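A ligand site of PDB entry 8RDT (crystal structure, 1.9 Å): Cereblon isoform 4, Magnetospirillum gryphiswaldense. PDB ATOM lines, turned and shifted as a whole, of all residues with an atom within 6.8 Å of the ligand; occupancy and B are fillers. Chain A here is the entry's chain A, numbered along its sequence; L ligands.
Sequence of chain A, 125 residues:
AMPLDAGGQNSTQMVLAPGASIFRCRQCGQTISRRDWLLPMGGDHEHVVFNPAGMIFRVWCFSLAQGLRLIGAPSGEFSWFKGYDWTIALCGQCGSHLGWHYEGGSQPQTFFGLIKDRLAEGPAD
O of Phe 78 lies within hydrogen-bond range of N1 of the ligand (2.8 Å).
OH of Tyr 102 lies within hydrogen-bond range of O3 of the ligand (2.8 Å).
The backbone NH (N) of Trp 80 lies within hydrogen-bond range of an oxygen (O3) of the ligand, 3.2 Å away.
The side-chain hydroxyl of Ser 79 sits at hydrogen-bond distance from the backbone carbonyl oxygen of Phe 81, 3.0 Å away.
The side-chain amide oxygen of Asn 51 is in hydrogen-bond range of the backbone NH of Ala 53, 2.9 Å away.
The indole nitrogen (NE1) of Trp 80 is in hydrogen-bond range of the backbone carbonyl oxygen (O) of Phe 50.
The side-chain amide oxygen (OD1) of Asn 51 sits at hydrogen-bond distance from the backbone NH (N) of Met 55.
OG of Ser 75 is in hydrogen-bond range of N of Glu 77, 3.2 Å away.
NE1 of Trp 86 lies within hydrogen-bond range of O of Glu 77, at 2.8 Å.
The backbone carbonyl oxygen of Ser 75 lies within hydrogen-bond range of the backbone NH of Trp 86 (2.7 Å).
The side-chain hydroxyl of Ser 79 is in hydrogen-bond range of the backbone carbonyl oxygen of Tyr 84 (2.8 Å).
Asn 51 touches the ligand.
Pro 52 touches the ligand.
Glu 77 touches the ligand (OE1 to C14, 3.98 Å).
Ser 79 touches the ligand.
Trp 86 touches the ligand (CZ2 to C16, 3.6 Å).
Trp 100 touches the ligand (NE1 to C6, 3.5 Å).
Hydrophobic or aromatic side chains that line the ligand: Pro 52, Phe 78, Trp 80, Trp 86, Trp 100 and Tyr 102.
Nine residues have an atom within 4 Å of the ligand: Asn 51, Pro 52, Glu 77, Phe 78, Ser 79, Trp 80, Trp 86, Trp 100 and Tyr 102.
The nearest printed residue that does not touch the ligand is Ala 53 (4.4 Å).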
ATOM      1  N   VAL A  49     -11.428   6.440  34.078  1.00  0.00           N
ATOM      2  CA  VAL A  49     -11.696   6.952  32.697  1.00  0.00           C
ATOM      3  C   VAL A  49     -11.300   5.874  31.675  1.00  0.00           C
ATOM      4  O   VAL A  49     -10.523   4.995  32.040  1.00  0.00           O
ATOM      5  CB  VAL A  49     -10.960   8.284  32.455  1.00  0.00           C
ATOM      6  CG1 VAL A  49     -11.537   9.365  33.358  1.00  0.00           C
ATOM      7  CG2 VAL A  49      -9.470   8.163  32.655  1.00  0.00           C
ATOM      8  N   PHE A  50     -11.783   5.989  30.431  1.00  0.00           N
ATOM      9  CA  PHE A  50     -11.296   5.182  29.293  1.00  0.00           C
ATOM     10  C   PHE A  50     -10.916   6.091  28.121  1.00  0.00           C
ATOM     11  O   PHE A  50     -11.555   7.155  27.914  1.00  0.00           O
ATOM     12  CB  PHE A  50     -12.298   4.113  28.897  1.00  0.00           C
ATOM     13  CG  PHE A  50     -13.601   4.582  28.334  1.00  0.00           C
ATOM     14  CD1 PHE A  50     -14.653   4.920  29.174  1.00  0.00           C
ATOM     15  CD2 PHE A  50     -13.840   4.521  26.960  1.00  0.00           C
ATOM     16  CE1 PHE A  50     -15.899   5.255  28.645  1.00  0.00           C
ATOM     17  CE2 PHE A  50     -15.083   4.843  26.435  1.00  0.00           C
ATOM     18  CZ  PHE A  50     -16.101   5.229  27.281  1.00  0.00           C
ATOM     19  N   ASN A  51      -9.867   5.683  27.387  1.00  0.00           N
ATOM     20  CA  ASN A  51      -9.384   6.405  26.179  1.00  0.00           C
ATOM     21  C   ASN A  51     -10.082   5.813  24.953  1.00  0.00           C
ATOM     22  O   ASN A  51     -10.883   4.878  25.050  1.00  0.00           O
ATOM     23  CB  ASN A  51      -7.845   6.419  26.163  1.00  0.00           C
ATOM     24  CG  ASN A  51      -7.215   5.093  25.806  1.00  0.00           C
ATOM     25  OD1 ASN A  51      -7.895   4.115  25.470  1.00  0.00           O
ATOM     26  ND2 ASN A  51      -5.897   5.057  25.898  1.00  0.00           N
ATOM     27  N   PRO A  52      -9.890   6.386  23.751  1.00  0.00           N
ATOM     28  CA  PRO A  52     -10.513   5.841  22.543  1.00  0.00           C
ATOM     29  C   PRO A  52      -9.983   4.452  22.161  1.00  0.00           C
ATOM     30  O   PRO A  52     -10.570   3.848  21.338  1.00  0.00           O
ATOM     31  CB  PRO A  52     -10.189   6.873  21.460  1.00  0.00           C
ATOM     32  CG  PRO A  52      -9.790   8.135  22.212  1.00  0.00           C
ATOM     33  CD  PRO A  52      -9.171   7.645  23.505  1.00  0.00           C
ATOM     34  N   ALA A  53      -8.850   4.003  22.710  1.00  0.00           N
ATOM     35  CA  ALA A  53      -8.309   2.628  22.536  1.00  0.00           C
ATOM     36  C   ALA A  53      -8.843   1.661  23.667  1.00  0.00           C
ATOM     37  O   ALA A  53      -8.367   0.528  23.690  1.00  0.00           O
ATOM     38  CB  ALA A  53      -6.798   2.621  22.526  1.00  0.00           C
ATOM     39  N   MET A  55      -8.835   1.544  26.725  1.00  0.00           N
ATOM     40  CA  MET A  55      -7.988   1.298  27.896  1.00  0.00           C
ATOM     41  C   MET A  55      -8.574   2.095  29.062  1.00  0.00           C
ATOM     42  O   MET A  55      -8.858   3.316  28.906  1.00  0.00           O
ATOM     43  CB  MET A  55      -6.562   1.791  27.642  1.00  0.00           C
ATOM     44  CG  MET A  55      -5.889   1.106  26.469  1.00  0.00           C
ATOM     45  SD  MET A  55      -4.178   1.642  26.322  1.00  0.00           S
ATOM     46  CE  MET A  55      -3.534   1.036  27.886  1.00  0.00           C
ATOM     47  N   PHE A  57      -8.196   3.511  32.871  1.00  0.00           N
ATOM     48  CA  PHE A  57      -7.168   3.991  33.823  1.00  0.00           C
ATOM     49  C   PHE A  57      -7.879   4.469  35.074  1.00  0.00           C
ATOM     50  O   PHE A  57      -8.950   5.121  34.985  1.00  0.00           O
ATOM     51  CB  PHE A  57      -6.330   5.124  33.229  1.00  0.00           C
ATOM     52  CG  PHE A  57      -5.683   4.857  31.900  1.00  0.00           C
ATOM     53  CD1 PHE A  57      -4.425   4.276  31.823  1.00  0.00           C
ATOM     54  CD2 PHE A  57      -6.298   5.220  30.716  1.00  0.00           C
ATOM     55  CE1 PHE A  57      -3.808   4.076  30.600  1.00  0.00           C
ATOM     56  CE2 PHE A  57      -5.683   5.002  29.485  1.00  0.00           C
ATOM     57  CZ  PHE A  57      -4.433   4.442  29.437  1.00  0.00           C
ATOM     58  N   SER A  75      -2.533  18.955  24.078  1.00  0.00           N
ATOM     59  CA  SER A  75      -3.685  18.704  23.173  1.00  0.00           C
ATOM     60  C   SER A  75      -4.956  18.671  24.022  1.00  0.00           C
ATOM     61  O   SER A  75      -4.916  18.148  25.135  1.00  0.00           O
ATOM     62  CB  SER A  75      -3.490  17.385  22.426  1.00  0.00           C
ATOM     63  OG  SER A  75      -4.662  17.094  21.666  1.00  0.00           O
ATOM     64  N   GLY A  76      -6.059  19.203  23.500  1.00  0.00           N
ATOM     65  CA  GLY A  76      -7.368  19.112  24.147  1.00  0.00           C
ATOM     66  C   GLY A  76      -8.143  17.872  23.714  1.00  0.00           C
ATOM     67  O   GLY A  76      -9.182  17.596  24.315  1.00  0.00           O
ATOM     68  N   GLU A  77      -7.681  17.168  22.674  1.00  0.00           N
ATOM     69  CA  GLU A  77      -8.440  16.064  22.007  1.00  0.00           C
ATOM     70  C   GLU A  77      -8.758  14.971  23.028  1.00  0.00           C
ATOM     71  O   GLU A  77      -7.828  14.501  23.664  1.00  0.00           O
ATOM     72  CB  GLU A  77      -7.616  15.451  20.872  1.00  0.00           C
ATOM     73  CG  GLU A  77      -7.285  16.457  19.795  1.00  0.00           C
ATOM     74  CD  GLU A  77      -6.774  15.876  18.494  1.00  0.00           C
ATOM     75  OE1 GLU A  77      -6.088  14.825  18.537  1.00  0.00           O
ATOM     76  OE2 GLU A  77      -7.065  16.486  17.441  1.00  0.00           O
ATOM     77  N   PHE A  78     -10.033  14.623  23.230  1.00  0.00           N
ATOM     78  CA  PHE A  78     -10.480  13.529  24.123  1.00  0.00           C
ATOM     79  C   PHE A  78     -10.058  13.804  25.578  1.00  0.00           C
ATOM     80  O   PHE A  78     -10.001  12.836  26.347  1.00  0.00           O
ATOM     81  CB  PHE A  78      -9.885  12.183  23.698  1.00  0.00           C
ATOM     82  CG  PHE A  78     -10.163  11.805  22.254  1.00  0.00           C
ATOM     83  CD1 PHE A  78     -11.428  11.435  21.870  1.00  0.00           C
ATOM     84  CD2 PHE A  78      -9.151  11.771  21.320  1.00  0.00           C
ATOM     85  CE1 PHE A  78     -11.694  11.073  20.556  1.00  0.00           C
ATOM     86  CE2 PHE A  78      -9.398  11.402  20.017  1.00  0.00           C
ATOM     87  CZ  PHE A  78     -10.675  11.044  19.633  1.00  0.00           C
ATOM     88  N   SER A  79      -9.832  15.043  25.972  1.00  0.00           N
ATOM     89  CA  SER A  79      -9.517  15.380  27.372  1.00  0.00           C
ATOM     90  C   SER A  79     -10.670  14.930  28.271  1.00  0.00           C
ATOM     91  O   SER A  79     -11.809  15.243  27.975  1.00  0.00           O
ATOM     92  CB  SER A  79      -9.223  16.841  27.599  1.00  0.00           C
ATOM     93  OG  SER A  79      -8.938  17.036  28.979  1.00  0.00           O
ATOM     94  N   TRP A  80     -10.356  14.240  29.371  1.00  0.00           N
ATOM     95  CA  TRP A  80     -11.330  13.769  30.382  1.00  0.00           C
ATOM     96  C   TRP A  80     -11.765  14.918  31.286  1.00  0.00           C
ATOM     97  O   TRP A  80     -12.782  14.777  31.973  1.00  0.00           O
ATOM     98  CB  TRP A  80     -10.736  12.657  31.222  1.00  0.00           C
ATOM     99  CG  TRP A  80     -10.450  11.424  30.428  1.00  0.00           C
ATOM    100  CD1 TRP A  80     -11.307  10.750  29.603  1.00  0.00           C
ATOM    101  CD2 TRP A  80      -9.205  10.719  30.407  1.00  0.00           C
ATOM    102  NE1 TRP A  80     -10.671   9.648  29.092  1.00  0.00           N
ATOM    103  CE2 TRP A  80      -9.379   9.615  29.552  1.00  0.00           C
ATOM    104  CE3 TRP A  80      -7.966  10.912  31.021  1.00  0.00           C
ATOM    105  CZ2 TRP A  80      -8.356   8.714  29.301  1.00  0.00           C
ATOM    106  CZ3 TRP A  80      -6.956  10.014  30.768  1.00  0.00           C
ATOM    107  CH2 TRP A  80      -7.155   8.917  29.931  1.00  0.00           C
ATOM    108  N   PHE A  81     -10.996  15.995  31.324  1.00  0.00           N
ATOM    109  CA  PHE A  81     -11.233  17.117  32.248  1.00  0.00           C
ATOM    110  C   PHE A  81     -11.542  18.345  31.426  1.00  0.00           C
ATOM    111  O   PHE A  81     -10.645  18.826  30.712  1.00  0.00           O
ATOM    112  CB  PHE A  81     -10.033  17.300  33.165  1.00  0.00           C
ATOM    113  CG  PHE A  81      -9.703  16.070  33.961  1.00  0.00           C
ATOM    114  CD1 PHE A  81     -10.383  15.816  35.130  1.00  0.00           C
ATOM    115  CD2 PHE A  81      -8.721  15.200  33.559  1.00  0.00           C
ATOM    116  CE1 PHE A  81     -10.056  14.729  35.928  1.00  0.00           C
ATOM    117  CE2 PHE A  81      -8.412  14.089  34.341  1.00  0.00           C
ATOM    118  CZ  PHE A  81      -9.068  13.864  35.538  1.00  0.00           C
ATOM    119  N   TYR A  84      -9.258  21.569  30.130  1.00  0.00           N
ATOM    120  CA  TYR A  84      -7.831  21.224  30.258  1.00  0.00           C
ATOM    121  C   TYR A  84      -7.299  20.486  29.027  1.00  0.00           C
ATOM    122  O   TYR A  84      -7.972  19.589  28.511  1.00  0.00           O
ATOM    123  CB  TYR A  84      -7.550  20.397  31.498  1.00  0.00           C
ATOM    124  CG  TYR A  84      -7.895  21.071  32.785  1.00  0.00           C
ATOM    125  CD1 TYR A  84      -6.955  21.850  33.449  1.00  0.00           C
ATOM    126  CD2 TYR A  84      -9.111  20.845  33.406  1.00  0.00           C
ATOM    127  CE1 TYR A  84      -7.243  22.440  34.657  1.00  0.00           C
ATOM    128  CE2 TYR A  84      -9.437  21.463  34.614  1.00  0.00           C
ATOM    129  CZ  TYR A  84      -8.493  22.276  35.228  1.00  0.00           C
ATOM    130  OH  TYR A  84      -8.744  22.820  36.453  1.00  0.00           O
ATOM    131  N   TRP A  86      -3.919  18.202  27.669  1.00  0.00           N
ATOM    132  CA  TRP A  86      -3.017  17.204  28.280  1.00  0.00           C
ATOM    133  C   TRP A  86      -1.700  17.137  27.515  1.00  0.00           C
ATOM    134  O   TRP A  86      -1.669  17.358  26.286  1.00  0.00           O
ATOM    135  CB  TRP A  86      -3.673  15.802  28.383  1.00  0.00           C
ATOM    136  CG  TRP A  86      -4.246  15.331  27.094  1.00  0.00           C
ATOM    137  CD1 TRP A  86      -5.532  15.489  26.649  1.00  0.00           C
ATOM    138  CD2 TRP A  86      -3.527  14.697  26.013  1.00  0.00           C
ATOM    139  NE1 TRP A  86      -5.648  15.011  25.374  1.00  0.00           N
ATOM    140  CE2 TRP A  86      -4.451  14.516  24.954  1.00  0.00           C
ATOM    141  CE3 TRP A  86      -2.207  14.276  25.830  1.00  0.00           C
ATOM    142  CZ2 TRP A  86      -4.095  13.927  23.744  1.00  0.00           C
ATOM    143  CZ3 TRP A  86      -1.861  13.668  24.641  1.00  0.00           C
ATOM    144  CH2 TRP A  86      -2.798  13.513  23.604  1.00  0.00           C
ATOM    145  N   ILE A  88       1.454  14.101  27.618  1.00  0.00           N
ATOM    146  CA  ILE A  88       1.885  12.765  28.100  1.00  0.00           C
ATOM    147  C   ILE A  88       3.042  12.987  29.091  1.00  0.00           C
ATOM    148  O   ILE A  88       3.991  13.788  28.779  1.00  0.00           O
ATOM    149  CB  ILE A  88       2.310  11.859  26.934  1.00  0.00           C
ATOM    150  CG1 ILE A  88       1.119  11.555  26.011  1.00  0.00           C
ATOM    151  CG2 ILE A  88       2.943  10.585  27.482  1.00  0.00           C
ATOM    152  CD1 ILE A  88       1.512  11.136  24.612  1.00  0.00           C
ATOM    153  N   HIS A  97       5.056   5.128  30.883  1.00  0.00           N
ATOM    154  CA  HIS A  97       3.955   6.114  30.801  1.00  0.00           C
ATOM    155  C   HIS A  97       3.245   6.185  32.166  1.00  0.00           C
ATOM    156  O   HIS A  97       2.661   5.184  32.559  1.00  0.00           O
ATOM    157  CB  HIS A  97       3.000   5.756  29.653  1.00  0.00           C
ATOM    158  CG  HIS A  97       1.845   6.697  29.591  1.00  0.00           C
ATOM    159  ND1 HIS A  97       0.599   6.293  29.151  1.00  0.00           N
ATOM    160  CD2 HIS A  97       1.730   8.004  29.921  1.00  0.00           C
ATOM    161  CE1 HIS A  97      -0.222   7.334  29.173  1.00  0.00           C
ATOM    162  NE2 HIS A  97       0.453   8.389  29.658  1.00  0.00           N
ATOM    163  N   TRP A 100      -0.509  12.037  32.696  1.00  0.00           N
ATOM    164  CA  TRP A 100      -0.617  13.296  31.910  1.00  0.00           C
ATOM    165  C   TRP A 100      -0.457  14.500  32.842  1.00  0.00           C
ATOM    166  O   TRP A 100      -0.868  14.437  34.015  1.00  0.00           O
ATOM    167  CB  TRP A 100      -1.930  13.347  31.125  1.00  0.00           C
ATOM    168  CG  TRP A 100      -2.182  12.105  30.331  1.00  0.00           C
ATOM    169  CD1 TRP A 100      -1.888  11.903  29.021  1.00  0.00           C
ATOM    170  CD2 TRP A 100      -2.753  10.864  30.806  1.00  0.00           C
ATOM    171  NE1 TRP A 100      -2.220  10.622  28.656  1.00  0.00           N
ATOM    172  CE2 TRP A 100      -2.775   9.973  29.727  1.00  0.00           C
ATOM    173  CE3 TRP A 100      -3.252  10.432  32.040  1.00  0.00           C
ATOM    174  CZ2 TRP A 100      -3.267   8.667  29.834  1.00  0.00           C
ATOM    175  CZ3 TRP A 100      -3.737   9.140  32.163  1.00  0.00           C
ATOM    176  CH2 TRP A 100      -3.709   8.267  31.076  1.00  0.00           C
ATOM    177  N   TYR A 102      -1.961  18.280  32.937  1.00  0.00           N
ATOM    178  CA  TYR A 102      -3.134  19.047  32.456  1.00  0.00           C
ATOM    179  C   TYR A 102      -2.848  20.525  32.672  1.00  0.00           C
ATOM    180  O   TYR A 102      -2.310  20.863  33.729  1.00  0.00           O
ATOM    181  CB  TYR A 102      -4.392  18.578  33.164  1.00  0.00           C
ATOM    182  CG  TYR A 102      -4.843  17.220  32.714  1.00  0.00           C
ATOM    183  CD1 TYR A 102      -5.644  17.060  31.591  1.00  0.00           C
ATOM    184  CD2 TYR A 102      -4.421  16.077  33.384  1.00  0.00           C
ATOM    185  CE1 TYR A 102      -6.046  15.805  31.167  1.00  0.00           C
ATOM    186  CE2 TYR A 102      -4.828  14.808  32.968  1.00  0.00           C
ATOM    187  CZ  TYR A 102      -5.638  14.679  31.855  1.00  0.00           C
ATOM    188  OH  TYR A 102      -6.007  13.428  31.387  1.00  0.00           O
HETATM  189  C1  LIG L   1      -5.526  11.981  28.148  1.00  0.00           C
HETATM  190  O1  LIG L   1      -6.015   7.865  19.318  1.00  0.00           O
HETATM  191  C2  LIG L   1      -6.972  12.361  28.243  1.00  0.00           C
HETATM  192  C3  LIG L   1      -7.558  10.619  26.607  1.00  0.00           C
HETATM  193  C4  LIG L   1      -6.083  11.000  24.658  1.00  0.00           C
HETATM  194  C5  LIG L   1      -6.096  10.484  26.091  1.00  0.00           C
HETATM  195  C6  LIG L   1      -5.080  11.363  26.827  1.00  0.00           C
HETATM  196  O2  LIG L   1      -5.460  10.294  18.233  1.00  0.00           O
HETATM  197  O3  LIG L   1      -7.359  13.276  28.939  1.00  0.00           O
HETATM  198  N1  LIG L   1      -7.857  11.555  27.570  1.00  0.00           N
HETATM  199  O4  LIG L   1      -8.445   9.940  26.120  1.00  0.00           O
HETATM  200  O5  LIG L   1      -5.590   9.097  25.932  1.00  0.00           O
HETATM  201  N2  LIG L   1      -5.579   8.732  24.537  1.00  0.00           N
HETATM  202  C7  LIG L   1      -5.719   9.789  23.842  1.00  0.00           C
HETATM  203  C8  LIG L   1      -5.603   9.875  22.370  1.00  0.00           C
HETATM  204  C9  LIG L   1      -5.862   8.786  21.509  1.00  0.00           C
HETATM  205  O6  LIG L   1      -6.124   7.547  22.003  1.00  0.00           O
HETATM  206  C10 LIG L   1      -5.012   6.643  22.098  1.00  0.00           C
HETATM  207  C11 LIG L   1      -5.787   8.961  20.124  1.00  0.00           C
HETATM  208  C12 LIG L   1      -7.263   7.898  18.626  1.00  0.00           C
HETATM  209  C13 LIG L   1      -5.503  10.225  19.592  1.00  0.00           C
HETATM  210  C14 LIG L   1      -6.504  10.987  17.556  1.00  0.00           C
HETATM  211  C15 LIG L   1      -5.295  11.305  20.440  1.00  0.00           C
HETATM  212  C16 LIG L   1      -5.349  11.137  21.803  1.00  0.00           C
